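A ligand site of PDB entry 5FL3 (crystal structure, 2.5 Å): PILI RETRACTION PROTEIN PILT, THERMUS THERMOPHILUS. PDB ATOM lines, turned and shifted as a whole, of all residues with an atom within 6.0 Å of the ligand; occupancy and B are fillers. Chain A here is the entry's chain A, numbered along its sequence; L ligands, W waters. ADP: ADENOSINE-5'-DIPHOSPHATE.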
ATOM      1  N   ARG A  23     -14.663  -2.605  -3.755  1.00  0.00           N
ATOM      2  CA  ARG A  23     -14.105  -1.272  -3.428  1.00  0.00           C
ATOM      3  C   ARG A  23     -15.023  -0.393  -2.576  1.00  0.00           C
ATOM      4  O   ARG A  23     -15.012   0.836  -2.691  1.00  0.00           O
ATOM      5  CB  ARG A  23     -13.712  -0.509  -4.699  1.00  0.00           C
ATOM      6  CG  ARG A  23     -12.411  -1.004  -5.325  1.00  0.00           C
ATOM      7  CD  ARG A  23     -12.116  -0.218  -6.579  1.00  0.00           C
ATOM      8  NE  ARG A  23     -13.293  -0.173  -7.448  1.00  0.00           N
ATOM      9  CZ  ARG A  23     -13.926   0.959  -7.764  1.00  0.00           C
ATOM     10  NH1 ARG A  23     -13.491   2.116  -7.288  1.00  0.00           N
ATOM     11  NH2 ARG A  23     -14.989   0.913  -8.564  1.00  0.00           N
ATOM     12  N   SER A  25     -16.014   1.789   0.268  1.00  0.00           N
ATOM     13  CA  SER A  25     -15.429   2.618   1.296  1.00  0.00           C
ATOM     14  C   SER A  25     -16.244   2.530   2.590  1.00  0.00           C
ATOM     15  O   SER A  25     -15.703   2.650   3.694  1.00  0.00           O
ATOM     16  CB  SER A  25     -15.326   4.048   0.817  1.00  0.00           C
ATOM     17  OG  SER A  25     -16.596   4.468   0.375  1.00  0.00           O
ATOM     18  N   ASP A  26     -17.550   2.335   2.437  1.00  0.00           N
ATOM     19  CA  ASP A  26     -18.482   2.376   3.562  1.00  0.00           C
ATOM     20  C   ASP A  26     -19.583   1.353   3.367  1.00  0.00           C
ATOM     21  O   ASP A  26     -20.096   1.178   2.245  1.00  0.00           O
ATOM     22  CB  ASP A  26     -19.097   3.769   3.726  1.00  0.00           C
ATOM     23  CG  ASP A  26     -18.058   4.875   3.879  1.00  0.00           C
ATOM     24  OD1 ASP A  26     -17.610   5.461   2.851  1.00  0.00           O
ATOM     25  OD2 ASP A  26     -17.681   5.169   5.032  1.00  0.00           O
ATOM     26  N   ASP A  40     -17.071   4.655  -4.898  1.00  0.00           N
ATOM     27  CA  ASP A  40     -16.748   5.893  -5.621  1.00  0.00           C
ATOM     28  C   ASP A  40     -17.647   7.064  -5.209  1.00  0.00           C
ATOM     29  O   ASP A  40     -18.096   7.828  -6.064  1.00  0.00           O
ATOM     30  CB  ASP A  40     -16.833   5.692  -7.144  1.00  0.00           C
ATOM     31  CG  ASP A  40     -15.856   4.641  -7.666  1.00  0.00           C
ATOM     32  OD1 ASP A  40     -14.731   4.567  -7.124  1.00  0.00           O
ATOM     33  OD2 ASP A  40     -16.229   3.880  -8.592  1.00  0.00           O
ATOM     34  N   GLY A  41     -17.908   7.181  -3.912  1.00  0.00           N
ATOM     35  CA  GLY A  41     -18.651   8.302  -3.359  1.00  0.00           C
ATOM     36  C   GLY A  41     -20.150   8.091  -3.357  1.00  0.00           C
ATOM     37  O   GLY A  41     -20.871   8.823  -2.680  1.00  0.00           O
ATOM     38  N   ALA A 117      -2.254   7.002 -10.098  1.00  0.00           N
ATOM     39  CA  ALA A 117      -3.615   6.541  -9.817  1.00  0.00           C
ATOM     40  C   ALA A 117      -4.545   7.673  -9.370  1.00  0.00           C
ATOM     41  O   ALA A 117      -5.702   7.723  -9.763  1.00  0.00           O
ATOM     42  CB  ALA A 117      -3.593   5.449  -8.782  1.00  0.00           C
ATOM     43  N   LEU A 118      -4.029   8.592  -8.549  1.00  0.00           N
ATOM     44  CA  LEU A 118      -4.866   9.637  -7.966  1.00  0.00           C
ATOM     45  C   LEU A 118      -5.039  10.834  -8.890  1.00  0.00           C
ATOM     46  O   LEU A 118      -5.822  11.732  -8.590  1.00  0.00           O
ATOM     47  CB  LEU A 118      -4.267  10.112  -6.636  1.00  0.00           C
ATOM     48  CG  LEU A 118      -4.234   9.012  -5.567  1.00  0.00           C
ATOM     49  CD1 LEU A 118      -3.729   9.539  -4.231  1.00  0.00           C
ATOM     50  CD2 LEU A 118      -5.610   8.374  -5.455  1.00  0.00           C
ATOM     51  N   GLY A 119      -4.306  10.838 -10.004  1.00  0.00           N
ATOM     52  CA  GLY A 119      -4.278  11.992 -10.876  1.00  0.00           C
ATOM     53  C   GLY A 119      -3.592  13.207 -10.262  1.00  0.00           C
ATOM     54  O   GLY A 119      -3.991  14.339 -10.537  1.00  0.00           O
ATOM     55  N   LEU A 120      -2.581  12.961  -9.424  1.00  0.00           N
ATOM     56  CA  LEU A 120      -1.786  14.008  -8.780  1.00  0.00           C
ATOM     57  C   LEU A 120      -0.436  14.114  -9.479  1.00  0.00           C
ATOM     58  O   LEU A 120       0.283  13.109  -9.580  1.00  0.00           O
ATOM     59  CB  LEU A 120      -1.560  13.711  -7.294  1.00  0.00           C
ATOM     60  CG  LEU A 120      -2.647  13.547  -6.235  1.00  0.00           C
ATOM     61  CD1 LEU A 120      -2.117  12.683  -5.103  1.00  0.00           C
ATOM     62  CD2 LEU A 120      -3.017  14.892  -5.674  1.00  0.00           C
ATOM     63  N   GLY A 140     -10.840  21.180   0.297  1.00  0.00           N
ATOM     64  CA  GLY A 140     -12.003  20.693  -0.411  1.00  0.00           C
ATOM     65  C   GLY A 140     -13.048  20.171   0.566  1.00  0.00           C
ATOM     66  O   GLY A 140     -12.740  19.911   1.730  1.00  0.00           O
ATOM     67  N   PRO A 141     -14.301  20.017   0.114  1.00  0.00           N
ATOM     68  CA  PRO A 141     -15.307  19.522   1.065  1.00  0.00           C
ATOM     69  C   PRO A 141     -15.206  18.012   1.242  1.00  0.00           C
ATOM     70  O   PRO A 141     -14.493  17.369   0.479  1.00  0.00           O
ATOM     71  CB  PRO A 141     -16.631  19.931   0.396  1.00  0.00           C
ATOM     72  CG  PRO A 141     -16.321  19.890  -1.078  1.00  0.00           C
ATOM     73  CD  PRO A 141     -14.884  20.319  -1.214  1.00  0.00           C
ATOM     74  N   THR A 142     -15.892  17.450   2.239  1.00  0.00           N
ATOM     75  CA  THR A 142     -15.951  15.990   2.407  1.00  0.00           C
ATOM     76  C   THR A 142     -16.093  15.268   1.083  1.00  0.00           C
ATOM     77  O   THR A 142     -16.929  15.645   0.279  1.00  0.00           O
ATOM     78  CB  THR A 142     -17.123  15.559   3.286  1.00  0.00           C
ATOM     79  OG1 THR A 142     -16.937  16.078   4.599  1.00  0.00           O
ATOM     80  CG2 THR A 142     -17.194  14.039   3.340  1.00  0.00           C
ATOM     81  N   GLY A 143     -15.277  14.242   0.873  1.00  0.00           N
ATOM     82  CA  GLY A 143     -15.411  13.415  -0.309  1.00  0.00           C
ATOM     83  C   GLY A 143     -14.610  13.908  -1.491  1.00  0.00           C
ATOM     84  O   GLY A 143     -14.863  13.514  -2.620  1.00  0.00           O
ATOM     85  N   SER A 144     -13.625  14.754  -1.219  1.00  0.00           N
ATOM     86  CA  SER A 144     -12.812  15.337  -2.282  1.00  0.00           C
ATOM     87  C   SER A 144     -11.491  14.607  -2.489  1.00  0.00           C
ATOM     88  O   SER A 144     -10.700  14.999  -3.348  1.00  0.00           O
ATOM     89  CB  SER A 144     -12.522  16.804  -1.982  1.00  0.00           C
ATOM     90  OG  SER A 144     -13.730  17.556  -2.038  1.00  0.00           O
ATOM     91  N   GLY A 145     -11.247  13.564  -1.692  1.00  0.00           N
ATOM     92  CA  GLY A 145      -9.993  12.837  -1.757  1.00  0.00           C
ATOM     93  C   GLY A 145      -8.831  13.473  -1.027  1.00  0.00           C
ATOM     94  O   GLY A 145      -7.665  13.273  -1.389  1.00  0.00           O
ATOM     95  N   LYS A 146      -9.136  14.236   0.022  1.00  0.00           N
ATOM     96  CA  LYS A 146      -8.109  14.935   0.798  1.00  0.00           C
ATOM     97  C   LYS A 146      -7.287  13.936   1.615  1.00  0.00           C
ATOM     98  O   LYS A 146      -6.057  13.989   1.584  1.00  0.00           O
ATOM     99  CB  LYS A 146      -8.744  15.998   1.688  1.00  0.00           C
ATOM    100  CG  LYS A 146      -9.496  17.069   0.911  1.00  0.00           C
ATOM    101  CD  LYS A 146      -9.836  18.260   1.768  1.00  0.00           C
ATOM    102  CE  LYS A 146     -10.721  17.877   2.930  1.00  0.00           C
ATOM    103  NZ  LYS A 146     -12.017  17.307   2.440  1.00  0.00           N
ATOM    104  N   SER A 147      -7.968  13.007   2.302  1.00  0.00           N
ATOM    105  CA  SER A 147      -7.312  11.935   3.062  1.00  0.00           C
ATOM    106  C   SER A 147      -6.346  11.132   2.203  1.00  0.00           C
ATOM    107  O   SER A 147      -5.288  10.680   2.649  1.00  0.00           O
ATOM    108  CB  SER A 147      -8.350  10.980   3.656  1.00  0.00           C
ATOM    109  OG  SER A 147      -9.289  11.663   4.439  1.00  0.00           O
ATOM    110  N   THR A 148      -6.756  10.936   0.955  1.00  0.00           N
ATOM    111  CA  THR A 148      -6.061  10.078   0.024  1.00  0.00           C
ATOM    112  C   THR A 148      -4.836  10.781  -0.523  1.00  0.00           C
ATOM    113  O   THR A 148      -3.754  10.211  -0.606  1.00  0.00           O
ATOM    114  CB  THR A 148      -6.983   9.649  -1.123  1.00  0.00           C
ATOM    115  OG1 THR A 148      -8.163   9.035  -0.585  1.00  0.00           O
ATOM    116  CG2 THR A 148      -6.285   8.661  -1.992  1.00  0.00           C
ATOM    117  N   THR A 149      -4.997  12.043  -0.891  1.00  0.00           N
ATOM    118  CA  THR A 149      -3.836  12.774  -1.332  1.00  0.00           C
ATOM    119  C   THR A 149      -2.801  12.780  -0.212  1.00  0.00           C
ATOM    120  O   THR A 149      -1.616  12.504  -0.462  1.00  0.00           O
ATOM    121  CB  THR A 149      -4.211  14.163  -1.754  1.00  0.00           C
ATOM    122  OG1 THR A 149      -4.977  14.060  -2.962  1.00  0.00           O
ATOM    123  CG2 THR A 149      -2.962  14.990  -1.992  1.00  0.00           C
ATOM    124  N   GLU A 173      -7.746   7.069   8.510  1.00  0.00           N
ATOM    125  CA  GLU A 173      -8.350   6.589   7.263  1.00  0.00           C
ATOM    126  C   GLU A 173      -7.439   5.576   6.574  1.00  0.00           C
ATOM    127  O   GLU A 173      -7.909   4.621   5.962  1.00  0.00           O
ATOM    128  CB  GLU A 173      -8.673   7.757   6.320  1.00  0.00           C
ATOM    129  CG  GLU A 173      -9.711   8.787   6.843  1.00  0.00           C
ATOM    130  CD  GLU A 173     -11.134   8.229   6.863  1.00  0.00           C
ATOM    131  OE1 GLU A 173     -11.332   7.076   6.398  1.00  0.00           O
ATOM    132  OE2 GLU A 173     -12.057   8.940   7.378  1.00  0.00           O
ATOM    133  N   PHE A 174      -6.131   5.802   6.677  1.00  0.00           N
ATOM    134  CA  PHE A 174      -5.126   4.912   6.100  1.00  0.00           C
ATOM    135  C   PHE A 174      -4.122   4.465   7.158  1.00  0.00           C
ATOM    136  O   PHE A 174      -3.696   5.277   7.988  1.00  0.00           O
ATOM    137  CB  PHE A 174      -4.378   5.609   4.963  1.00  0.00           C
ATOM    138  CG  PHE A 174      -5.202   5.800   3.750  1.00  0.00           C
ATOM    139  CD1 PHE A 174      -5.250   4.806   2.772  1.00  0.00           C
ATOM    140  CD2 PHE A 174      -5.937   6.954   3.560  1.00  0.00           C
ATOM    141  CE1 PHE A 174      -6.015   4.977   1.650  1.00  0.00           C
ATOM    142  CE2 PHE A 174      -6.703   7.125   2.438  1.00  0.00           C
ATOM    143  CZ  PHE A 174      -6.746   6.142   1.479  1.00  0.00           C
ATOM    144  N   GLN A 276      -9.081  20.418  -4.136  1.00  0.00           N
ATOM    145  CA  GLN A 276      -9.506  19.245  -4.873  1.00  0.00           C
ATOM    146  C   GLN A 276     -11.011  19.154  -5.006  1.00  0.00           C
ATOM    147  O   GLN A 276     -11.745  19.574  -4.122  1.00  0.00           O
ATOM    148  CB  GLN A 276      -8.970  17.989  -4.199  1.00  0.00           C
ATOM    149  CG  GLN A 276      -7.463  17.906  -4.237  1.00  0.00           C
ATOM    150  CD  GLN A 276      -6.938  16.611  -3.685  1.00  0.00           C
ATOM    151  OE1 GLN A 276      -7.684  15.683  -3.404  1.00  0.00           O
ATOM    152  NE2 GLN A 276      -5.634  16.543  -3.531  1.00  0.00           N
ATOM    153  N   LEU A 278     -13.716  16.037  -6.766  1.00  0.00           N
ATOM    154  CA  LEU A 278     -13.834  14.761  -7.477  1.00  0.00           C
ATOM    155  C   LEU A 278     -15.060  14.753  -8.383  1.00  0.00           C
ATOM    156  O   LEU A 278     -16.191  14.773  -7.891  1.00  0.00           O
ATOM    157  CB  LEU A 278     -13.923  13.592  -6.501  1.00  0.00           C
ATOM    158  CG  LEU A 278     -12.606  13.208  -5.860  1.00  0.00           C
ATOM    159  CD1 LEU A 278     -12.808  12.117  -4.820  1.00  0.00           C
ATOM    160  CD2 LEU A 278     -11.675  12.742  -6.948  1.00  0.00           C
ATOM    161  N   ARG A 287     -14.523   8.170 -10.865  1.00  0.00           N
ATOM    162  CA  ARG A 287     -14.329   9.616 -10.744  1.00  0.00           C
ATOM    163  C   ARG A 287     -12.911  10.045 -11.085  1.00  0.00           C
ATOM    164  O   ARG A 287     -11.996   9.233 -11.162  1.00  0.00           O
ATOM    165  CB  ARG A 287     -14.685  10.098  -9.339  1.00  0.00           C
ATOM    166  CG  ARG A 287     -16.134   9.925  -8.998  1.00  0.00           C
ATOM    167  CD  ARG A 287     -16.495  10.637  -7.723  1.00  0.00           C
ATOM    168  NE  ARG A 287     -15.852  10.029  -6.559  1.00  0.00           N
ATOM    169  CZ  ARG A 287     -16.018  10.460  -5.311  1.00  0.00           C
ATOM    170  NH1 ARG A 287     -16.825  11.478  -5.068  1.00  0.00           N
ATOM    171  NH2 ARG A 287     -15.397   9.849  -4.298  1.00  0.00           N
ATOM    172  N   VAL A 288     -12.743  11.342 -11.290  1.00  0.00           N
ATOM    173  CA  VAL A 288     -11.467  11.915 -11.681  1.00  0.00           C
ATOM    174  C   VAL A 288     -11.222  13.183 -10.846  1.00  0.00           C
ATOM    175  O   VAL A 288     -12.173  13.863 -10.416  1.00  0.00           O
ATOM    176  CB  VAL A 288     -11.451  12.203 -13.208  1.00  0.00           C
ATOM    177  CG1 VAL A 288     -12.626  13.082 -13.587  1.00  0.00           C
ATOM    178  CG2 VAL A 288     -10.147  12.820 -13.648  1.00  0.00           C
ATOM    179  N   LEU A 289      -9.951  13.492 -10.596  1.00  0.00           N
ATOM    180  CA  LEU A 289      -9.601  14.611  -9.746  1.00  0.00           C
ATOM    181  C   LEU A 289      -9.419  15.904 -10.531  1.00  0.00           C
ATOM    182  O   LEU A 289      -8.643  15.980 -11.492  1.00  0.00           O
ATOM    183  CB  LEU A 289      -8.334  14.295  -8.930  1.00  0.00           C
ATOM    184  CG  LEU A 289      -7.796  15.373  -7.978  1.00  0.00           C
ATOM    185  CD1 LEU A 289      -8.809  15.767  -6.923  1.00  0.00           C
ATOM    186  CD2 LEU A 289      -6.515  14.892  -7.294  1.00  0.00           C
HETATM  187  PB  ADP L   1     -11.954  13.435   1.895  1.00  0.00           P
HETATM  188  O1B ADP L   1     -13.293  13.161   2.570  1.00  0.00           O
HETATM  189  O2B ADP L   1     -11.887  14.752   1.151  1.00  0.00           O
HETATM  190  O3B ADP L   1     -10.757  13.185   2.770  1.00  0.00           O
HETATM  191  PA  ADP L   1     -11.328  10.812   0.801  1.00  0.00           P
HETATM  192  O1A ADP L   1     -11.985  10.158   2.011  1.00  0.00           O
HETATM  193  O2A ADP L   1      -9.828  10.673   0.566  1.00  0.00           O
HETATM  194  O3A ADP L   1     -11.832  12.351   0.707  1.00  0.00           O
HETATM  195  O5' ADP L   1     -12.031  10.240  -0.537  1.00  0.00           O
HETATM  196  C5' ADP L   1     -13.404   9.857  -0.608  1.00  0.00           C
HETATM  197  C4' ADP L   1     -13.497   8.769  -1.679  1.00  0.00           C
HETATM  198  O4' ADP L   1     -12.926   9.240  -2.911  1.00  0.00           O
HETATM  199  C3' ADP L   1     -12.765   7.499  -1.296  1.00  0.00           C
HETATM  200  O3' ADP L   1     -13.685   6.428  -1.499  1.00  0.00           O
HETATM  201  C2' ADP L   1     -11.569   7.415  -2.248  1.00  0.00           C
HETATM  202  O2' ADP L   1     -11.334   6.086  -2.735  1.00  0.00           O
HETATM  203  C1' ADP L   1     -11.940   8.327  -3.402  1.00  0.00           C
HETATM  204  N9  ADP L   1     -10.766   9.079  -3.936  1.00  0.00           N
HETATM  205  C8  ADP L   1      -9.818   9.696  -3.204  1.00  0.00           C
HETATM  206  N7  ADP L   1      -8.879  10.306  -3.982  1.00  0.00           N
HETATM  207  C5  ADP L   1      -9.233  10.082  -5.265  1.00  0.00           C
HETATM  208  C6  ADP L   1      -8.693  10.446  -6.597  1.00  0.00           C
HETATM  209  N6  ADP L   1      -7.563  11.193  -6.680  1.00  0.00           N
HETATM  210  N1  ADP L   1      -9.368  10.012  -7.699  1.00  0.00           N
HETATM  211  C2  ADP L   1     -10.495   9.281  -7.610  1.00  0.00           C
HETATM  212  N3  ADP L   1     -11.052   8.923  -6.435  1.00  0.00           N
HETATM  213  C4  ADP L   1     -10.478   9.273  -5.243  1.00  0.00           C
HETATM  214  O   HOH W   1      -6.511  11.960  -3.878  1.00  0.00           O
HETATM  215  O   HOH W   2     -11.969  10.956   4.579  1.00  0.00           O
HETATM  216  O   HOH W   3     -14.759  11.079   2.622  1.00  0.00           O
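CB of Ser 25 touches O3' of the ligand, at 3.7 Å.
Pro 141 touches the ligand.
Thr 142 touches the ligand.
CD1 of Leu 278 touches O4' of the ligand, at 3.5 Å.
Leu 289 touches the ligand.
13 residues have an atom within 4 Å of the ligand: Ser 25, Leu 118, Pro 141, Thr 142, Gly 143, Ser 144, Gly 145, Lys 146, Ser 147, Thr 148, Leu 278, Arg 287 and Leu 289.
The nearest printed residue that does not touch the ligand is Gly 119 (4.7 Å).
Water W2 lies within hydrogen-bond range of an oxygen (O1A) of the ligand, the side-chain hydroxyl (OG) of Ser 147 and the side-chain carboxylate (OE2) of Glu 173.
Water W1 lies within hydrogen-bond range of the side-chain hydroxyl (OG1) of Thr 149 (2.8 Å), a nitrogen (N7) of the ligand (2.9 Å) and the backbone carbonyl oxygen (O) of Gly 145 (3.0 Å).
NE of Arg 287 is in hydrogen-bond range of O of Asp 40, 3.2 Å away.
The side-chain carboxylate of Asp 26 is in hydrogen-bond range of the side-chain hydroxyl of Ser 25 (2.9 Å).
The backbone carbonyl oxygen (O) of Gly 145 sits close to the side-chain amide oxygen (OE1) of Gln 276, at 3.1 Å.
O of Ser 144 sits close to OE1 of Gln 276 (3.1 Å).
The backbone carbonyl oxygen (O) of Pro 141 sits at hydrogen-bond distance from the side-chain hydroxyl (OG) of Ser 144 (2.6 Å).
NZ of Lys 146 is in hydrogen-bond range of O of Pro 141 (3.2 Å).
The backbone carbonyl oxygen of Gly 140 sits at hydrogen-bond distance from the side-chain amino group of Lys 146 (2.8 Å).
The backbone carbonyl oxygen (O) of Gly 145 lies within hydrogen-bond range of the side-chain hydroxyl (OG1) of Thr 149, at 3.2 Å.
OG of Ser 147 lies within hydrogen-bond range of O3B of the ligand.
The side-chain hydroxyl (OG1) of Thr 148 is in hydrogen-bond range of an oxygen (O2A) of the ligand, 2.6 Å away.
N of Gly 145 sits at hydrogen-bond distance from O3A of the ligand, at 2.8 Å.
O2B of the ligand sits at hydrogen-bond distance from N of Lys 146, 3.0 Å away.
The side-chain amino group (NZ) of Lys 146 is in salt-bridge range of an oxygen (O2B) of the ligand.
NH2 of Arg 287 lies within hydrogen-bond range of O4' of the ligand.
The backbone NH (N) of Thr 148 lies within hydrogen-bond range of an oxygen (O2A) of the ligand (3.1 Å).
N of Ser 147 lies within hydrogen-bond range of O3B of the ligand (2.8 Å).
An oxygen (O2B) of the ligand sits at hydrogen-bond distance from the backbone NH of Ser 144.
N of Gly 143 is in hydrogen-bond range of O1B of the ligand, at 2.8 Å.
The backbone carbonyl oxygen (O) of Leu 118 is in hydrogen-bond range of a nitrogen (N6) of the ligand (2.6 Å).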
